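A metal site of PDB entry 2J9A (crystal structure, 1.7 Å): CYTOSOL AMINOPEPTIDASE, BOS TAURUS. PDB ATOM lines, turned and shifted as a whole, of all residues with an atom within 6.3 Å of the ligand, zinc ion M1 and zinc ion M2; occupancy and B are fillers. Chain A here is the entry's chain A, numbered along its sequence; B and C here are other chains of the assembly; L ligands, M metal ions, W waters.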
ATOM      1  N   LYS A 250      17.027 -17.887  -5.263  1.00  0.00           N
ATOM      2  CA  LYS A 250      17.673 -18.524  -4.124  1.00  0.00           C
ATOM      3  C   LYS A 250      16.624 -19.132  -3.155  1.00  0.00           C
ATOM      4  O   LYS A 250      15.752 -18.403  -2.676  1.00  0.00           O
ATOM      5  CB  LYS A 250      18.539 -17.470  -3.402  1.00  0.00           C
ATOM      6  CG  LYS A 250      19.066 -17.924  -2.014  1.00  0.00           C
ATOM      7  CD  LYS A 250      19.852 -16.708  -1.341  1.00  0.00           C
ATOM      8  CE  LYS A 250      20.231 -17.107   0.093  1.00  0.00           C
ATOM      9  NZ  LYS A 250      20.786 -15.947   0.864  1.00  0.00           N
ATOM     10  N   ILE A 252      16.977 -20.751  -0.025  1.00  0.00           N
ATOM     11  CA  ILE A 252      17.469 -21.252   1.258  1.00  0.00           C
ATOM     12  C   ILE A 252      16.281 -21.223   2.249  1.00  0.00           C
ATOM     13  O   ILE A 252      15.822 -20.150   2.666  1.00  0.00           O
ATOM     14  CB  ILE A 252      18.627 -20.354   1.751  1.00  0.00           C
ATOM     15  CG1 ILE A 252      19.846 -20.570   0.826  1.00  0.00           C
ATOM     16  CG2 ILE A 252      18.965 -20.702   3.228  1.00  0.00           C
ATOM     17  CD1 ILE A 252      20.435 -22.035   0.879  1.00  0.00           C
ATOM     18  N   ASP A 255      18.365 -20.055   6.848  1.00  0.00           N
ATOM     19  CA  ASP A 255      19.822 -19.733   6.856  1.00  0.00           C
ATOM     20  C   ASP A 255      20.292 -19.454   8.309  1.00  0.00           C
ATOM     21  O   ASP A 255      20.051 -18.382   8.879  1.00  0.00           O
ATOM     22  CB  ASP A 255      20.101 -18.503   5.984  1.00  0.00           C
ATOM     23  CG  ASP A 255      21.594 -18.238   5.792  1.00  0.00           C
ATOM     24  OD1 ASP A 255      22.386 -19.120   6.172  1.00  0.00           O
ATOM     25  OD2 ASP A 255      21.913 -17.173   5.236  1.00  0.00           O
ATOM     26  N   SER A 256      20.965 -20.455   8.906  1.00  0.00           N
ATOM     27  CA  SER A 256      21.598 -20.262  10.220  1.00  0.00           C
ATOM     28  C   SER A 256      22.983 -19.603  10.052  1.00  0.00           C
ATOM     29  O   SER A 256      23.643 -19.279  11.072  1.00  0.00           O
ATOM     30  CB  SER A 256      21.808 -21.614  10.947  1.00  0.00           C
ATOM     31  OG  SER A 256      22.802 -22.369  10.230  1.00  0.00           O
ATOM     32  N   GLY A 257      23.414 -19.459   8.811  1.00  0.00           N
ATOM     33  CA  GLY A 257      24.827 -19.141   8.498  1.00  0.00           C
ATOM     34  C   GLY A 257      25.736 -20.354   8.330  1.00  0.00           C
ATOM     35  O   GLY A 257      26.809 -20.246   7.704  1.00  0.00           O
ATOM     36  N   LYS A 262      25.284 -17.339  12.327  1.00  0.00           N
ATOM     37  CA  LYS A 262      24.713 -15.994  12.602  1.00  0.00           C
ATOM     38  C   LYS A 262      24.500 -15.795  14.099  1.00  0.00           C
ATOM     39  O   LYS A 262      24.382 -16.760  14.840  1.00  0.00           O
ATOM     40  CB  LYS A 262      23.336 -15.875  11.918  1.00  0.00           C
ATOM     41  CG  LYS A 262      23.489 -15.780  10.380  1.00  0.00           C
ATOM     42  CD  LYS A 262      22.113 -15.746   9.731  1.00  0.00           C
ATOM     43  CE  LYS A 262      22.181 -15.593   8.176  1.00  0.00           C
ATOM     44  NZ  LYS A 262      23.030 -14.385   7.747  1.00  0.00           N
ATOM     45  N   LEU A 269      14.049 -14.404  11.121  1.00  0.00           N
ATOM     46  CA  LEU A 269      13.665 -13.838   9.784  1.00  0.00           C
ATOM     47  C   LEU A 269      14.301 -14.627   8.635  1.00  0.00           C
ATOM     48  O   LEU A 269      13.844 -14.500   7.471  1.00  0.00           O
ATOM     49  CB  LEU A 269      14.104 -12.383   9.665  1.00  0.00           C
ATOM     50  CG  LEU A 269      13.360 -11.476  10.680  1.00  0.00           C
ATOM     51  CD1 LEU A 269      13.966 -10.053  10.530  1.00  0.00           C
ATOM     52  CD2 LEU A 269      11.831 -11.467  10.472  1.00  0.00           C
ATOM     53  N   MET A 270      15.317 -15.428   8.951  1.00  0.00           N
ATOM     54  CA  MET A 270      15.997 -16.219   7.921  1.00  0.00           C
ATOM     55  C   MET A 270      15.135 -17.374   7.395  1.00  0.00           C
ATOM     56  O   MET A 270      15.538 -18.057   6.449  1.00  0.00           O
ATOM     57  CB  MET A 270      17.369 -16.736   8.394  1.00  0.00           C
ATOM     58  CG  MET A 270      18.413 -15.585   8.627  1.00  0.00           C
ATOM     59  SD  MET A 270      18.673 -14.589   7.096  1.00  0.00           S
ATOM     60  CE  MET A 270      17.493 -13.245   7.265  1.00  0.00           C
ATOM     61  N   ASP A 273      14.665 -16.706   3.731  1.00  0.00           N
ATOM     62  CA  ASP A 273      15.842 -16.721   2.849  1.00  0.00           C
ATOM     63  C   ASP A 273      15.573 -17.509   1.579  1.00  0.00           C
ATOM     64  O   ASP A 273      16.481 -17.675   0.783  1.00  0.00           O
ATOM     65  CB  ASP A 273      17.051 -17.290   3.567  1.00  0.00           C
ATOM     66  CG  ASP A 273      18.365 -16.713   3.036  1.00  0.00           C
ATOM     67  OD1 ASP A 273      18.356 -15.612   2.452  1.00  0.00           O
ATOM     68  OD2 ASP A 273      19.363 -17.409   3.262  1.00  0.00           O
ATOM     69  N   ASN A 305      20.643 -24.164   5.347  1.00  0.00           N
ATOM     70  CA  ASN A 305      22.069 -23.893   5.636  1.00  0.00           C
ATOM     71  C   ASN A 305      22.260 -24.052   7.140  1.00  0.00           C
ATOM     72  O   ASN A 305      21.909 -23.139   7.910  1.00  0.00           O
ATOM     73  CB  ASN A 305      22.497 -22.469   5.154  1.00  0.00           C
ATOM     74  CG  ASN A 305      24.024 -22.266   5.219  1.00  0.00           C
ATOM     75  OD1 ASN A 305      24.805 -23.240   5.112  1.00  0.00           O
ATOM     76  ND2 ASN A 305      24.457 -21.004   5.331  1.00  0.00           N
ATOM     77  N   THR A 331      30.739 -19.494   5.256  1.00  0.00           N
ATOM     78  CA  THR A 331      29.648 -20.439   4.903  1.00  0.00           C
ATOM     79  C   THR A 331      28.282 -19.749   4.903  1.00  0.00           C
ATOM     80  O   THR A 331      27.278 -20.378   4.493  1.00  0.00           O
ATOM     81  CB  THR A 331      29.574 -21.658   5.858  1.00  0.00           C
ATOM     82  OG1 THR A 331      29.192 -21.219   7.187  1.00  0.00           O
ATOM     83  CG2 THR A 331      30.912 -22.413   5.922  1.00  0.00           C
ATOM     84  N   ASP A 332      28.234 -18.496   5.344  1.00  0.00           N
ATOM     85  CA  ASP A 332      26.983 -17.734   5.367  1.00  0.00           C
ATOM     86  C   ASP A 332      26.807 -16.920   4.065  1.00  0.00           C
ATOM     87  O   ASP A 332      25.788 -16.278   3.859  1.00  0.00           O
ATOM     88  CB  ASP A 332      26.984 -16.802   6.587  1.00  0.00           C
ATOM     89  CG  ASP A 332      25.624 -16.189   6.924  1.00  0.00           C
ATOM     90  OD1 ASP A 332      24.554 -16.575   6.357  1.00  0.00           O
ATOM     91  OD2 ASP A 332      25.648 -15.283   7.804  1.00  0.00           O
ATOM     92  N   ALA A 333      27.816 -17.002   3.190  1.00  0.00           N
ATOM     93  CA  ALA A 333      27.662 -16.487   1.827  1.00  0.00           C
ATOM     94  C   ALA A 333      27.229 -17.685   0.937  1.00  0.00           C
ATOM     95  O   ALA A 333      27.877 -18.018  -0.060  1.00  0.00           O
ATOM     96  CB  ALA A 333      28.993 -15.844   1.315  1.00  0.00           C
ATOM     97  N   GLU A 334      26.154 -18.344   1.361  1.00  0.00           N
ATOM     98  CA  GLU A 334      25.725 -19.599   0.738  1.00  0.00           C
ATOM     99  C   GLU A 334      24.820 -19.352  -0.462  1.00  0.00           C
ATOM    100  O   GLU A 334      24.767 -20.204  -1.357  1.00  0.00           O
ATOM    101  CB  GLU A 334      25.011 -20.510   1.766  1.00  0.00           C
ATOM    102  CG  GLU A 334      23.470 -20.193   1.986  1.00  0.00           C
ATOM    103  CD  GLU A 334      23.198 -18.830   2.683  1.00  0.00           C
ATOM    104  OE1 GLU A 334      24.075 -18.381   3.457  1.00  0.00           O
ATOM    105  OE2 GLU A 334      22.122 -18.253   2.493  1.00  0.00           O
ATOM    106  N   GLY A 335      24.108 -18.240  -0.482  1.00  0.00           N
ATOM    107  CA  GLY A 335      23.223 -17.943  -1.647  1.00  0.00           C
ATOM    108  C   GLY A 335      23.983 -17.894  -2.951  1.00  0.00           C
ATOM    109  O   GLY A 335      23.547 -18.433  -4.010  1.00  0.00           O
ATOM    110  N   THR A 359      17.575 -13.087  -1.565  1.00  0.00           N
ATOM    111  CA  THR A 359      17.730 -12.298  -0.314  1.00  0.00           C
ATOM    112  C   THR A 359      19.239 -12.390   0.049  1.00  0.00           C
ATOM    113  O   THR A 359      19.622 -13.118   0.949  1.00  0.00           O
ATOM    114  CB  THR A 359      16.838 -12.898   0.786  1.00  0.00           C
ATOM    115  OG1 THR A 359      16.963 -14.325   0.734  1.00  0.00           O
ATOM    116  CG2 THR A 359      15.331 -12.508   0.576  1.00  0.00           C
ATOM    117  N   LEU A 360      20.098 -11.726  -0.728  1.00  0.00           N
ATOM    118  CA  LEU A 360      21.474 -12.216  -0.835  1.00  0.00           C
ATOM    119  C   LEU A 360      22.440 -11.646   0.221  1.00  0.00           C
ATOM    120  O   LEU A 360      23.333 -12.345   0.658  1.00  0.00           O
ATOM    121  CB  LEU A 360      22.040 -11.987  -2.267  1.00  0.00           C
ATOM    122  CG  LEU A 360      23.250 -12.872  -2.644  1.00  0.00           C
ATOM    123  CD1 LEU A 360      22.920 -14.369  -2.621  1.00  0.00           C
ATOM    124  CD2 LEU A 360      23.841 -12.437  -4.030  1.00  0.00           C
ATOM    125  N   THR A 361      22.308 -10.348   0.506  1.00  0.00           N
ATOM    126  CA  THR A 361      23.329  -9.741   1.347  1.00  0.00           C
ATOM    127  C   THR A 361      22.761  -8.802   2.362  1.00  0.00           C
ATOM    128  O   THR A 361      21.833  -8.062   2.074  1.00  0.00           O
ATOM    129  CB  THR A 361      24.406  -8.964   0.476  1.00  0.00           C
ATOM    130  OG1 THR A 361      23.819  -7.846  -0.194  1.00  0.00           O
ATOM    131  CG2 THR A 361      25.076  -9.870  -0.593  1.00  0.00           C
ATOM    132  N   GLY A 362      23.370  -8.772   3.558  1.00  0.00           N
ATOM    133  CA  GLY A 362      23.048  -7.732   4.531  1.00  0.00           C
ATOM    134  C   GLY A 362      23.440  -6.386   3.976  1.00  0.00           C
ATOM    135  O   GLY A 362      22.773  -5.359   4.288  1.00  0.00           O
ATOM    136  N   ALA A 363      24.464  -6.364   3.134  1.00  0.00           N
ATOM    137  CA  ALA A 363      24.964  -5.099   2.582  1.00  0.00           C
ATOM    138  C   ALA A 363      23.893  -4.392   1.749  1.00  0.00           C
ATOM    139  O   ALA A 363      23.783  -3.153   1.738  1.00  0.00           O
ATOM    140  CB  ALA A 363      26.196  -5.340   1.733  1.00  0.00           C
ATOM    141  N   ASP A 365      20.679  -4.361   2.354  1.00  0.00           N
ATOM    142  CA  ASP A 365      19.799  -3.687   3.293  1.00  0.00           C
ATOM    143  C   ASP A 365      20.462  -2.408   3.817  1.00  0.00           C
ATOM    144  O   ASP A 365      19.839  -1.352   3.914  1.00  0.00           O
ATOM    145  CB  ASP A 365      19.483  -4.597   4.496  1.00  0.00           C
ATOM    146  CG  ASP A 365      18.539  -3.918   5.435  1.00  0.00           C
ATOM    147  OD1 ASP A 365      17.437  -3.566   4.971  1.00  0.00           O
ATOM    148  OD2 ASP A 365      18.964  -3.571   6.539  1.00  0.00           O
ATOM    149  N   ALA A 451      17.264  -8.613  -0.349  1.00  0.00           N
ATOM    150  CA  ALA A 451      17.419  -8.698   1.116  1.00  0.00           C
ATOM    151  C   ALA A 451      16.792  -7.502   1.844  1.00  0.00           C
ATOM    152  O   ALA A 451      16.192  -7.654   2.925  1.00  0.00           O
ATOM    153  CB  ALA A 451      18.938  -8.825   1.518  1.00  0.00           C
ATOM    154  N   GLY A 452      16.912  -6.299   1.279  1.00  0.00           N
ATOM    155  CA  GLY A 452      16.348  -5.113   1.950  1.00  0.00           C
ATOM    156  C   GLY A 452      14.813  -5.006   1.890  1.00  0.00           C
ATOM    157  O   GLY A 452      14.211  -4.358   2.721  1.00  0.00           O
ATOM    158  N   MET A 454      12.842  -7.722   1.981  1.00  0.00           N
ATOM    159  CA  MET A 454      12.315  -9.001   2.492  1.00  0.00           C
ATOM    160  C   MET A 454      11.127  -8.813   3.452  1.00  0.00           C
ATOM    161  O   MET A 454      10.182  -9.626   3.445  1.00  0.00           O
ATOM    162  CB  MET A 454      13.445  -9.766   3.218  1.00  0.00           C
ATOM    163  CG  MET A 454      13.313 -11.286   3.259  1.00  0.00           C
ATOM    164  SD  MET A 454      14.742 -11.996   4.132  1.00  0.00           S
ATOM    165  CE  MET A 454      14.501 -11.213   5.741  1.00  0.00           C
ATOM    166  N   THR A 455      11.189  -7.770   4.270  1.00  0.00           N
ATOM    167  CA  THR A 455      10.149  -7.516   5.285  1.00  0.00           C
ATOM    168  C   THR A 455       9.533  -6.125   5.102  1.00  0.00           C
ATOM    169  O   THR A 455      10.097  -5.252   4.408  1.00  0.00           O
ATOM    170  CB  THR A 455      10.732  -7.575   6.734  1.00  0.00           C
ATOM    171  OG1 THR A 455      11.603  -6.441   6.916  1.00  0.00           O
ATOM    172  CG2 THR A 455      11.519  -8.850   6.960  1.00  0.00           C
ATOM    173  N   ALA B   1      24.973 -13.101   3.104  1.00  0.00           N
ATOM    174  CA  ALA B   1      26.329 -12.744   3.491  1.00  0.00           C
ATOM    175  C   ALA B   1      26.315 -11.545   4.424  1.00  0.00           C
ATOM    176  O   ALA B   1      25.582 -10.600   4.149  1.00  0.00           O
ATOM    177  CB  ALA B   1      27.192 -12.417   2.245  1.00  0.00           C
ATOM    178  N   MLE B   2      27.150 -11.605   5.481  1.00  0.00           N
ATOM    179  CN  MLE B   2      27.996 -12.806   5.660  1.00  0.00           C
ATOM    180  CA  MLE B   2      27.199 -10.433   6.418  1.00  0.00           C
ATOM    181  CB  MLE B   2      26.961 -10.873   7.856  1.00  0.00           C
ATOM    182  CG  MLE B   2      25.545 -11.529   7.968  1.00  0.00           C
ATOM    183  CD1 MLE B   2      25.240 -11.884   9.425  1.00  0.00           C
ATOM    184  CD2 MLE B   2      24.409 -10.653   7.418  1.00  0.00           C
ATOM    185  C   MLE B   2      28.481  -9.577   6.099  1.00  0.00           C
ATOM    186  O   MLE B   2      29.328 -10.016   5.301  1.00  0.00           O
ATOM    187  N   ARG C 425      18.651   0.789  11.128  1.00  0.00           N
ATOM    188  CA  ARG C 425      19.987   0.725  10.578  1.00  0.00           C
ATOM    189  C   ARG C 425      20.005   0.755   9.048  1.00  0.00           C
ATOM    190  O   ARG C 425      20.988   1.155   8.414  1.00  0.00           O
ATOM    191  CB  ARG C 425      20.773  -0.510  11.075  1.00  0.00           C
ATOM    192  CG  ARG C 425      20.072  -1.864  10.769  1.00  0.00           C
ATOM    193  CD  ARG C 425      21.003  -2.931  10.113  1.00  0.00           C
ATOM    194  NE  ARG C 425      20.213  -3.914   9.339  1.00  0.00           N
ATOM    195  CZ  ARG C 425      20.704  -4.927   8.610  1.00  0.00           C
ATOM    196  NH1 ARG C 425      19.870  -5.735   7.969  1.00  0.00           N
ATOM    197  NH2 ARG C 425      22.005  -5.158   8.521  1.00  0.00           N
ATOM    198  N   SER C 426      18.875   0.427   8.444  1.00  0.00           N
ATOM    199  CA  SER C 426      18.873   0.193   6.991  1.00  0.00           C
ATOM    200  C   SER C 426      19.022   1.498   6.232  1.00  0.00           C
ATOM    201  O   SER C 426      18.505   2.518   6.660  1.00  0.00           O
ATOM    202  CB  SER C 426      17.528  -0.414   6.609  1.00  0.00           C
ATOM    203  OG  SER C 426      17.341  -1.598   7.392  1.00  0.00           O
HETATM  204  C1  LIG L   1      16.768  -8.066   7.505  1.00  0.00           C
HETATM  205  C2  LIG L   1      17.401  -7.703   6.146  1.00  0.00           C
HETATM  206  C3  LIG L   1      18.852  -8.233   5.966  1.00  0.00           C
HETATM  207  C4  LIG L   1      18.902  -9.767   5.866  1.00  0.00           C
HETATM  208  C5  LIG L   1      20.186 -10.210   5.115  1.00  0.00           C
HETATM  209  C6  LIG L   1      20.230 -11.750   5.004  1.00  0.00           C
HETATM  210  C7  LIG L   1      21.378 -12.208   4.124  1.00  0.00           C
HETATM  211  C8  LIG L   1      21.618 -13.735   4.244  1.00  0.00           C
HETATM  212  N1  LIG L   1      20.445 -14.506   3.692  1.00  0.00           N
HETATM  213  C9  LIG L   1      22.826 -14.104   3.378  1.00  0.00           C
HETATM  214  O1  LIG L   1      23.004 -15.498   3.311  1.00  0.00           O
HETATM  215  C10 LIG L   1      24.147 -13.629   3.975  1.00  0.00           C
HETATM  216  O2  LIG L   1      24.358 -13.771   5.179  1.00  0.00           O
HETATM  217 ZN    ZN M   1      21.113 -16.449   2.921  1.00  0.00          ZN
HETATM  218 ZN    ZN M   2      23.790 -16.745   4.593  1.00  0.00          ZN
HETATM  219  O   HOH W   1      23.780 -15.869   0.814  1.00  0.00           O
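A nitrogen (N1) of the ligand sits close to the backbone carbonyl oxygen (O) of Thr 359, 3.2 Å away.
An oxygen (O2) of the ligand lies within hydrogen-bond range of the side-chain amino group (NZ) of Lys 262 (3.0 Å).
A carbon (C10) of the ligand is covalently linked to the backbone NH (N) of Ala 1 of chain B (1.3 Å).
Three residues have an atom within 4 Å of zinc ion M2: Asp 255, Asp 332 and Glu 334.
Within 4 Å of zinc ion M1: Lys 250, Asp 255, Asp 273 and Glu 334.
Along chain A the residues within 4 Å of zinc ion M1 span positions 250 to 334.
The nearest printed residue that does not touch zinc ion M1 is Thr 359 (4.1 Å).
Merely in contact with the ligand: Met 270, Leu 360, Gly 362, Asp 365, Ala 451, MLE 2 of chain B and Arg 425 of chain C.
The nearest printed residue that does not touch the ligand is Thr 361 (4.02 Å).
OD1 of Asp 332 is bound to zinc ion M2, at 1.9 Å.
Zinc ion M2 is bound by O1 of the ligand.
OE1 of Glu 334 is bound to zinc ion M2, at 2.0 Å.
The side-chain carboxylate (OD2) of Asp 255 is bound to zinc ion M2 (2.0 Å).
Zinc ion M2 is bound by the backbone carbonyl oxygen (O) of Asp 332, at 2.2 Å.
N of Asp 332 sits at hydrogen-bond distance from O of Gly 257.
N of Asp 255 is in hydrogen-bond range of O of Met 270 (3.5 Å).
OD2 of Asp 332 is in salt-bridge range of NZ of Lys 262 (2.8 Å).
The guanidinium group of Arg 425 of chain C is in salt-bridge range of the side-chain carboxylate of Asp 365.
The backbone carbonyl oxygen of Ala 1 of chain B sits at hydrogen-bond distance from the backbone NH of Gly 362 (2.9 Å).
O of Asp 273 sits at hydrogen-bond distance from N of Ile 252 (3.2 Å).
The side-chain carboxylate (OD1) of Asp 255 sits at hydrogen-bond distance from the backbone NH (N) of Gly 257, 2.9 Å away.
OD2 of Asp 255 sits close to NZ of Lys 262 (3.9 Å).
Zinc ion M1 is bound by OD2 of Asp 273 (2.0 Å), OE2 of Glu 334 (2.1 Å), NZ of Lys 250 (2.1 Å), O1 of the ligand (2.2 Å), N1 of the ligand (2.2 Å) and OD2 of Asp 255 (2.6 Å).
Zinc ion M1 has six donor atoms within binding distance.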
